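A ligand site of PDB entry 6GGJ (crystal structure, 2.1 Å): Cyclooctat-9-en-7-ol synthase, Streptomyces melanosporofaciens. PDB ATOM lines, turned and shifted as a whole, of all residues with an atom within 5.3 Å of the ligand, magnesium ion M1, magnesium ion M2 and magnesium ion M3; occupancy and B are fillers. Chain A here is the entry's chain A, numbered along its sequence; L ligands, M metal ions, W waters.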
ATOM      1  N   ASN A 103      -2.870  -1.453   3.729  1.00  0.00           N
ATOM      2  CA  ASN A 103      -4.179  -1.882   4.216  1.00  0.00           C
ATOM      3  C   ASN A 103      -4.713  -0.946   5.287  1.00  0.00           C
ATOM      4  O   ASN A 103      -5.895  -0.575   5.271  1.00  0.00           O
ATOM      5  CB  ASN A 103      -4.124  -3.310   4.735  1.00  0.00           C
ATOM      6  CG  ASN A 103      -5.477  -3.988   4.642  1.00  0.00           C
ATOM      7  OD1 ASN A 103      -6.145  -4.207   5.658  1.00  0.00           O
ATOM      8  ND2 ASN A 103      -5.906  -4.306   3.426  1.00  0.00           N
ATOM      9  N   THR A 106      -5.844   2.531   3.778  1.00  0.00           N
ATOM     10  CA  THR A 106      -7.070   2.453   2.975  1.00  0.00           C
ATOM     11  C   THR A 106      -8.279   2.121   3.846  1.00  0.00           C
ATOM     12  O   THR A 106      -9.397   2.524   3.515  1.00  0.00           O
ATOM     13  CB  THR A 106      -6.898   1.462   1.820  1.00  0.00           C
ATOM     14  OG1 THR A 106      -6.498   0.171   2.282  1.00  0.00           O
ATOM     15  CG2 THR A 106      -5.838   1.989   0.851  1.00  0.00           C
ATOM     16  N   PHE A 107      -8.065   1.460   4.986  1.00  0.00           N
ATOM     17  CA  PHE A 107      -9.108   1.372   6.014  1.00  0.00           C
ATOM     18  C   PHE A 107      -9.567   2.760   6.442  1.00  0.00           C
ATOM     19  O   PHE A 107     -10.772   3.047   6.494  1.00  0.00           O
ATOM     20  CB  PHE A 107      -8.583   0.580   7.208  1.00  0.00           C
ATOM     21  CG  PHE A 107      -9.182  -0.781   7.378  1.00  0.00           C
ATOM     22  CD1 PHE A 107     -10.517  -0.923   7.742  1.00  0.00           C
ATOM     23  CD2 PHE A 107      -8.403  -1.915   7.214  1.00  0.00           C
ATOM     24  CE1 PHE A 107     -11.072  -2.191   7.903  1.00  0.00           C
ATOM     25  CE2 PHE A 107      -8.948  -3.183   7.378  1.00  0.00           C
ATOM     26  CZ  PHE A 107     -10.281  -3.318   7.735  1.00  0.00           C
ATOM     27  N   ASP A 110     -11.686   4.228   3.969  1.00  0.00           N
ATOM     28  CA  ASP A 110     -12.994   3.572   3.929  1.00  0.00           C
ATOM     29  C   ASP A 110     -13.952   4.213   4.927  1.00  0.00           C
ATOM     30  O   ASP A 110     -15.124   4.467   4.602  1.00  0.00           O
ATOM     31  CB  ASP A 110     -12.826   2.078   4.211  1.00  0.00           C
ATOM     32  CG  ASP A 110     -14.109   1.285   3.979  1.00  0.00           C
ATOM     33  OD1 ASP A 110     -14.513   1.159   2.806  1.00  0.00           O
ATOM     34  OD2 ASP A 110     -14.697   0.791   4.957  1.00  0.00           O
ATOM     35  N   ASP A 111     -13.479   4.481   6.137  1.00  0.00           N
ATOM     36  CA  ASP A 111     -14.278   5.048   7.227  1.00  0.00           C
ATOM     37  C   ASP A 111     -14.450   6.565   7.145  1.00  0.00           C
ATOM     38  O   ASP A 111     -15.179   7.122   7.967  1.00  0.00           O
ATOM     39  CB  ASP A 111     -13.653   4.690   8.577  1.00  0.00           C
ATOM     40  CG  ASP A 111     -13.906   3.243   8.977  1.00  0.00           C
ATOM     41  OD1 ASP A 111     -15.025   2.741   8.715  1.00  0.00           O
ATOM     42  OD2 ASP A 111     -12.990   2.601   9.540  1.00  0.00           O
ATOM     43  N   PHE A 149      -8.594   1.300  -5.860  1.00  0.00           N
ATOM     44  CA  PHE A 149      -9.445   1.033  -4.705  1.00  0.00           C
ATOM     45  C   PHE A 149     -10.010   2.323  -4.088  1.00  0.00           C
ATOM     46  O   PHE A 149     -11.214   2.415  -3.810  1.00  0.00           O
ATOM     47  CB  PHE A 149      -8.693   0.248  -3.621  1.00  0.00           C
ATOM     48  CG  PHE A 149      -9.488   0.109  -2.358  1.00  0.00           C
ATOM     49  CD1 PHE A 149     -10.509  -0.839  -2.268  1.00  0.00           C
ATOM     50  CD2 PHE A 149      -9.262   0.953  -1.282  1.00  0.00           C
ATOM     51  CE1 PHE A 149     -11.270  -0.972  -1.136  1.00  0.00           C
ATOM     52  CE2 PHE A 149     -10.023   0.835  -0.120  1.00  0.00           C
ATOM     53  CZ  PHE A 149     -11.037  -0.135  -0.050  1.00  0.00           C
ATOM     54  N   ASP A 153     -13.948   3.441  -4.008  1.00  0.00           N
ATOM     55  CA  ASP A 153     -14.693   3.706  -2.785  1.00  0.00           C
ATOM     56  C   ASP A 153     -15.312   5.107  -2.822  1.00  0.00           C
ATOM     57  O   ASP A 153     -16.466   5.307  -2.446  1.00  0.00           O
ATOM     58  CB  ASP A 153     -13.770   3.518  -1.574  1.00  0.00           C
ATOM     59  CG  ASP A 153     -14.393   4.025  -0.283  1.00  0.00           C
ATOM     60  OD1 ASP A 153     -15.444   3.484   0.129  1.00  0.00           O
ATOM     61  OD2 ASP A 153     -13.808   4.958   0.354  1.00  0.00           O
ATOM     62  N   ARG A 177     -18.096  -6.456  -5.174  1.00  0.00           N
ATOM     63  CA  ARG A 177     -17.195  -6.567  -4.024  1.00  0.00           C
ATOM     64  C   ARG A 177     -15.796  -7.026  -4.396  1.00  0.00           C
ATOM     65  O   ARG A 177     -14.857  -6.760  -3.626  1.00  0.00           O
ATOM     66  CB  ARG A 177     -17.814  -7.506  -2.999  1.00  0.00           C
ATOM     67  CG  ARG A 177     -19.059  -6.880  -2.404  1.00  0.00           C
ATOM     68  CD  ARG A 177     -18.613  -5.684  -1.557  1.00  0.00           C
ATOM     69  NE  ARG A 177     -18.732  -5.976  -0.131  1.00  0.00           N
ATOM     70  CZ  ARG A 177     -18.010  -5.398   0.832  1.00  0.00           C
ATOM     71  NH1 ARG A 177     -17.112  -4.460   0.544  1.00  0.00           N
ATOM     72  NH2 ARG A 177     -18.190  -5.757   2.096  1.00  0.00           N
ATOM     73  N   ASP A 180     -14.584  -3.728  -4.461  1.00  0.00           N
ATOM     74  CA  ASP A 180     -14.951  -2.783  -3.416  1.00  0.00           C
ATOM     75  C   ASP A 180     -14.468  -3.234  -2.046  1.00  0.00           C
ATOM     76  O   ASP A 180     -14.064  -2.399  -1.216  1.00  0.00           O
ATOM     77  CB  ASP A 180     -16.442  -2.542  -3.386  1.00  0.00           C
ATOM     78  CG  ASP A 180     -16.866  -1.765  -2.164  1.00  0.00           C
ATOM     79  OD1 ASP A 180     -16.665  -0.533  -2.153  1.00  0.00           O
ATOM     80  OD2 ASP A 180     -17.362  -2.393  -1.205  1.00  0.00           O
ATOM     81  N   ILE A 181     -14.481  -4.546  -1.767  1.00  0.00           N
ATOM     82  CA  ILE A 181     -13.991  -4.998  -0.484  1.00  0.00           C
ATOM     83  C   ILE A 181     -12.475  -4.848  -0.383  1.00  0.00           C
ATOM     84  O   ILE A 181     -11.930  -4.864   0.720  1.00  0.00           O
ATOM     85  CB  ILE A 181     -14.426  -6.440  -0.169  1.00  0.00           C
ATOM     86  CG1 ILE A 181     -14.345  -6.666   1.347  1.00  0.00           C
ATOM     87  CG2 ILE A 181     -13.522  -7.446  -0.897  1.00  0.00           C
ATOM     88  CD1 ILE A 181     -15.063  -7.883   1.833  1.00  0.00           C
ATOM     89  N   GLY A 182     -11.789  -4.702  -1.511  1.00  0.00           N
ATOM     90  CA  GLY A 182     -10.348  -4.533  -1.503  1.00  0.00           C
ATOM     91  C   GLY A 182      -9.530  -5.774  -1.780  1.00  0.00           C
ATOM     92  O   GLY A 182      -8.287  -5.698  -1.711  1.00  0.00           O
ATOM     93  N   ASN A 220     -17.139 -10.880   6.403  1.00  0.00           N
ATOM     94  CA  ASN A 220     -17.194  -9.462   6.758  1.00  0.00           C
ATOM     95  C   ASN A 220     -18.613  -8.937   6.779  1.00  0.00           C
ATOM     96  O   ASN A 220     -18.976  -8.150   7.664  1.00  0.00           O
ATOM     97  CB  ASN A 220     -16.366  -8.633   5.775  1.00  0.00           C
ATOM     98  CG  ASN A 220     -16.541  -7.132   6.014  1.00  0.00           C
ATOM     99  OD1 ASN A 220     -17.364  -6.491   5.362  1.00  0.00           O
ATOM    100  ND2 ASN A 220     -15.793  -6.589   6.963  1.00  0.00           N
ATOM    101  N   ASP A 221     -19.438  -9.325   5.802  1.00  0.00           N
ATOM    102  CA  ASP A 221     -20.796  -8.814   5.770  1.00  0.00           C
ATOM    103  C   ASP A 221     -21.554  -9.200   7.026  1.00  0.00           C
ATOM    104  O   ASP A 221     -22.303  -8.393   7.585  1.00  0.00           O
ATOM    105  CB  ASP A 221     -21.530  -9.305   4.526  1.00  0.00           C
ATOM    106  CG  ASP A 221     -21.139  -8.540   3.277  1.00  0.00           C
ATOM    107  OD1 ASP A 221     -20.275  -7.647   3.373  1.00  0.00           O
ATOM    108  OD2 ASP A 221     -21.676  -8.878   2.195  1.00  0.00           O
ATOM    109  N   SER A 224     -20.100  -7.221  10.170  1.00  0.00           N
ATOM    110  CA  SER A 224     -20.174  -5.773  10.048  1.00  0.00           C
ATOM    111  C   SER A 224     -21.565  -5.296   9.646  1.00  0.00           C
ATOM    112  O   SER A 224     -21.755  -4.106   9.412  1.00  0.00           O
ATOM    113  CB  SER A 224     -19.124  -5.261   9.046  1.00  0.00           C
ATOM    114  OG  SER A 224     -19.553  -5.404   7.700  1.00  0.00           O
ATOM    115  N   ARG A 227     -23.005  -2.452  12.257  1.00  0.00           N
ATOM    116  CA  ARG A 227     -22.423  -1.127  12.044  1.00  0.00           C
ATOM    117  C   ARG A 227     -22.976  -0.478  10.783  1.00  0.00           C
ATOM    118  O   ARG A 227     -23.469   0.657  10.820  1.00  0.00           O
ATOM    119  CB  ARG A 227     -20.905  -1.214  11.962  1.00  0.00           C
ATOM    120  CG  ARG A 227     -20.301  -0.023  11.221  1.00  0.00           C
ATOM    121  CD  ARG A 227     -18.827   0.150  11.539  1.00  0.00           C
ATOM    122  NE  ARG A 227     -18.060  -1.077  11.319  1.00  0.00           N
ATOM    123  CZ  ARG A 227     -17.639  -1.499  10.122  1.00  0.00           C
ATOM    124  NH1 ARG A 227     -17.921  -0.802   9.026  1.00  0.00           N
ATOM    125  NH2 ARG A 227     -16.928  -2.611  10.031  1.00  0.00           N
ATOM    126  N   GLU A 228     -22.910  -1.186   9.648  1.00  0.00           N
ATOM    127  CA  GLU A 228     -23.236  -0.562   8.373  1.00  0.00           C
ATOM    128  C   GLU A 228     -24.719  -0.231   8.249  1.00  0.00           C
ATOM    129  O   GLU A 228     -25.078   0.769   7.616  1.00  0.00           O
ATOM    130  CB  GLU A 228     -22.753  -1.464   7.232  1.00  0.00           C
ATOM    131  CG  GLU A 228     -21.237  -1.733   7.316  1.00  0.00           C
ATOM    132  CD  GLU A 228     -20.721  -2.829   6.397  1.00  0.00           C
ATOM    133  OE1 GLU A 228     -21.537  -3.580   5.815  1.00  0.00           O
ATOM    134  OE2 GLU A 228     -19.477  -2.933   6.252  1.00  0.00           O
ATOM    135  N   GLN A 233     -25.300   2.150   5.347  1.00  0.00           N
ATOM    136  CA  GLN A 233     -24.485   1.605   4.270  1.00  0.00           C
ATOM    137  C   GLN A 233     -25.170   0.375   3.692  1.00  0.00           C
ATOM    138  O   GLN A 233     -25.664  -0.475   4.437  1.00  0.00           O
ATOM    139  CB  GLN A 233     -23.084   1.272   4.792  1.00  0.00           C
ATOM    140  CG  GLN A 233     -22.182   2.489   4.823  1.00  0.00           C
ATOM    141  CD  GLN A 233     -21.092   2.401   5.880  1.00  0.00           C
ATOM    142  OE1 GLN A 233     -21.313   1.876   6.961  1.00  0.00           O
ATOM    143  NE2 GLN A 233     -19.911   2.909   5.551  1.00  0.00           N
ATOM    144  N   THR A 235     -23.776  -1.746   1.282  1.00  0.00           N
ATOM    145  CA  THR A 235     -22.866  -2.735   0.690  1.00  0.00           C
ATOM    146  C   THR A 235     -22.696  -3.895   1.671  1.00  0.00           C
ATOM    147  O   THR A 235     -21.698  -4.024   2.376  1.00  0.00           O
ATOM    148  CB  THR A 235     -21.547  -2.078   0.323  1.00  0.00           C
ATOM    149  OG1 THR A 235     -21.816  -0.996  -0.578  1.00  0.00           O
ATOM    150  CG2 THR A 235     -20.607  -3.076  -0.356  1.00  0.00           C
ATOM    151  N   ASN A 236     -23.704  -4.773   1.689  1.00  0.00           N
ATOM    152  CA  ASN A 236     -23.705  -5.906   2.612  1.00  0.00           C
ATOM    153  C   ASN A 236     -24.751  -6.919   2.156  1.00  0.00           C
ATOM    154  O   ASN A 236     -25.934  -6.591   2.111  1.00  0.00           O
ATOM    155  CB  ASN A 236     -24.011  -5.437   4.026  1.00  0.00           C
ATOM    156  CG  ASN A 236     -23.808  -6.511   5.062  1.00  0.00           C
ATOM    157  OD1 ASN A 236     -24.513  -7.542   5.065  1.00  0.00           O
ATOM    158  ND2 ASN A 236     -22.848  -6.299   5.960  1.00  0.00           N
ATOM    159  N   ARG A 294     -13.079  -4.115  16.001  1.00  0.00           N
ATOM    160  CA  ARG A 294     -13.811  -3.414  14.954  1.00  0.00           C
ATOM    161  C   ARG A 294     -15.248  -3.889  14.853  1.00  0.00           C
ATOM    162  O   ARG A 294     -16.155  -3.094  14.568  1.00  0.00           O
ATOM    163  CB  ARG A 294     -13.099  -3.589  13.607  1.00  0.00           C
ATOM    164  CG  ARG A 294     -13.760  -2.783  12.471  1.00  0.00           C
ATOM    165  CD  ARG A 294     -12.843  -2.543  11.279  1.00  0.00           C
ATOM    166  NE  ARG A 294     -13.577  -1.978  10.151  1.00  0.00           N
ATOM    167  CZ  ARG A 294     -13.726  -0.675   9.915  1.00  0.00           C
ATOM    168  NH1 ARG A 294     -13.202   0.225  10.732  1.00  0.00           N
ATOM    169  NH2 ARG A 294     -14.416  -0.264   8.848  1.00  0.00           N
ATOM    170  N   TYR A 295     -15.502  -5.174  15.125  1.00  0.00           N
ATOM    171  CA  TYR A 295     -16.774  -5.799  14.760  1.00  0.00           C
ATOM    172  C   TYR A 295     -17.557  -6.306  15.971  1.00  0.00           C
ATOM    173  O   TYR A 295     -18.288  -7.297  15.861  1.00  0.00           O
ATOM    174  CB  TYR A 295     -16.551  -6.942  13.773  1.00  0.00           C
ATOM    175  CG  TYR A 295     -15.746  -6.555  12.563  1.00  0.00           C
ATOM    176  CD1 TYR A 295     -16.302  -5.760  11.553  1.00  0.00           C
ATOM    177  CD2 TYR A 295     -14.434  -6.969  12.414  1.00  0.00           C
ATOM    178  CE1 TYR A 295     -15.573  -5.394  10.444  1.00  0.00           C
ATOM    179  CE2 TYR A 295     -13.690  -6.617  11.296  1.00  0.00           C
ATOM    180  CZ  TYR A 295     -14.274  -5.823  10.306  1.00  0.00           C
ATOM    181  OH  TYR A 295     -13.543  -5.463   9.191  1.00  0.00           O
HETATM  182  C1  LIG L   1     -12.601  -3.359   4.202  1.00  0.00           C
HETATM  183  C2  LIG L   1     -11.546  -2.365   3.728  1.00  0.00           C
HETATM  184  C3  LIG L   1     -13.521  -2.625   5.175  1.00  0.00           C
HETATM  185  C4  LIG L   1     -14.780  -3.469   5.310  1.00  0.00           C
HETATM  186  O1  LIG L   1     -14.521  -3.282   8.001  1.00  0.00           O
HETATM  187  P1  LIG L   1     -15.588  -3.108   6.936  1.00  0.00           P
HETATM  188  O2  LIG L   1     -16.729  -4.055   7.194  1.00  0.00           O
HETATM  189  O3  LIG L   1     -16.150  -1.706   6.917  1.00  0.00           O
HETATM  190  P2  LIG L   1     -15.950  -3.067   3.946  1.00  0.00           P
HETATM  191  O4  LIG L   1     -15.405  -3.807   2.742  1.00  0.00           O
HETATM  192  O5  LIG L   1     -17.329  -3.562   4.328  1.00  0.00           O
HETATM  193  O6  LIG L   1     -16.033  -1.587   3.634  1.00  0.00           O
HETATM  194  O7  LIG L   1     -14.449  -4.826   5.197  1.00  0.00           O
HETATM  195  N1  LIG L   1     -10.431  -3.133   3.210  1.00  0.00           N
HETATM  196 MG    MG M   1     -16.390  -0.309   5.261  1.00  0.00          MG
HETATM  197 MG    MG M   2     -18.167  -4.526   5.816  1.00  0.00          MG
HETATM  198 MG    MG M   3     -15.961  -0.377   2.093  1.00  0.00          MG
HETATM  199  O   HOH W   1     -18.103  -0.678   5.813  1.00  0.00           O
HETATM  200  O   HOH W   2     -17.386   1.055   3.252  1.00  0.00           O
HETATM  201  O   HOH W   3     -17.837  -1.326   1.154  1.00  0.00           O
HETATM  202  O   HOH W   4     -14.432  -1.532   1.398  1.00  0.00           O
HETATM  203  O   HOH W   5     -12.377  -5.990   6.642  1.00  0.00           O
HETATM  204  O   HOH W   6     -16.891   1.574   6.789  1.00  0.00           O
HETATM  205  O   HOH W   7     -19.923  -5.433   4.739  1.00  0.00           O
HETATM  206  O   HOH W   8     -16.109   0.842   0.267  1.00  0.00           O
HETATM  207  O   HOH W   9     -19.253  -2.611   2.771  1.00  0.00           O
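The guanidinium group (NH2) of Arg 227 is in salt-bridge range of an oxygen (O1) of the ligand, 3.2 Å away. The side-chain hydroxyl (OH) of Tyr 295 is in hydrogen-bond range of an oxygen (O1) of the ligand. NH1 of Arg 177 is in salt-bridge range of O4 of the ligand, 2.9 Å away. NE of Arg 294 is in salt-bridge range of O1 of the ligand, 2.7 Å away. The backbone carbonyl oxygen (O) of Ile 181 sits at hydrogen-bond distance from a nitrogen (N1) of the ligand.
NH2 of Arg 177 lies within salt-bridge range of OD1 of Asp 221, 3.1 Å away. NH2 of Arg 177 sits close to OD1 of Asn 220 (3.4 Å). The guanidinium group (NH1) of Arg 227 sits close to the side-chain carboxylate (OE2) of Glu 228, 3.8 Å away. OD2 of Asp 111 is in salt-bridge range of NH1 of Arg 294 (2.7 Å). The backbone NH of Gln 233 lies within hydrogen-bond range of the backbone carbonyl oxygen of Glu 228, at 2.7 Å. The side-chain carboxylate (OE1) of Glu 228 sits at hydrogen-bond distance from the side-chain amide nitrogen (ND2) of Asn 236. NH1 of Arg 177 lies within salt-bridge range of OD2 of Asp 180. The side-chain hydroxyl (OH) of Tyr 295 lies within hydrogen-bond range of the side-chain amide nitrogen (ND2) of Asn 220 (3.4 Å).
Merely in contact with the ligand: Phe 107 (3.6 Å).
The nearest printed residue that does not touch magnesium ion M1 is Arg 227 (4.1 Å).
NH2 of Arg 177 touches magnesium ion M2, at 3.9 Å.
Of the 21 residues printed, 1 comes within 4 Å of magnesium ion M3. The nearest printed residue that does not touch magnesium ion M3 is Asp 180 (4.1 Å).
Magnesium ion M1 is bound by water W1 (1.8 Å), OD2 of Asp 110 (2.0 Å), O6 of the ligand (2.1 Å), O3 of the ligand (2.2 Å) and water W6 (2.5 Å). Slightly farther from magnesium ion M1 lies water W2 (2.6 Å).
Magnesium ion M2 is bound by an oxygen (O5) of the ligand, an oxygen (O2) of the ligand, the side-chain carboxylate (OE2) of Glu 228, the side-chain amide oxygen (OD1) of Asn 220, water W7 and the side-chain hydroxyl (OG) of Ser 224. Magnesium ion M2 has six donor atoms within binding distance.
Magnesium ion M3 is bound by an oxygen (O6) of the ligand, water W4, water W8, the side-chain carboxylate of Asp 110, water W3 and water W2. Magnesium ion M3 has six donor atoms within binding distance.
Water W6 bridges the side-chain carboxylate of Asp 111 (2.9 Å) and the guanidinium group of Arg 227 (3.4 Å). Water W8 lies within hydrogen-bond range of OD1 of Asp 153 and OD1 of Asp 180. Water W3 bridges OD2 of Asp 180 (2.6 Å) and NH1 of Arg 177 (3.3 Å). Water W4 lies within hydrogen-bond range of the backbone carbonyl oxygen (O) of Asp 180 (2.8 Å) and an oxygen (O4) of the ligand (2.8 Å). Water W9 bridges O of Thr 235 (2.9 Å) and NH2 of Arg 177 (3.4 Å). Water W5 lies within hydrogen-bond range of O7 of the ligand, OH of Tyr 295 and ND2 of Asn 220.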
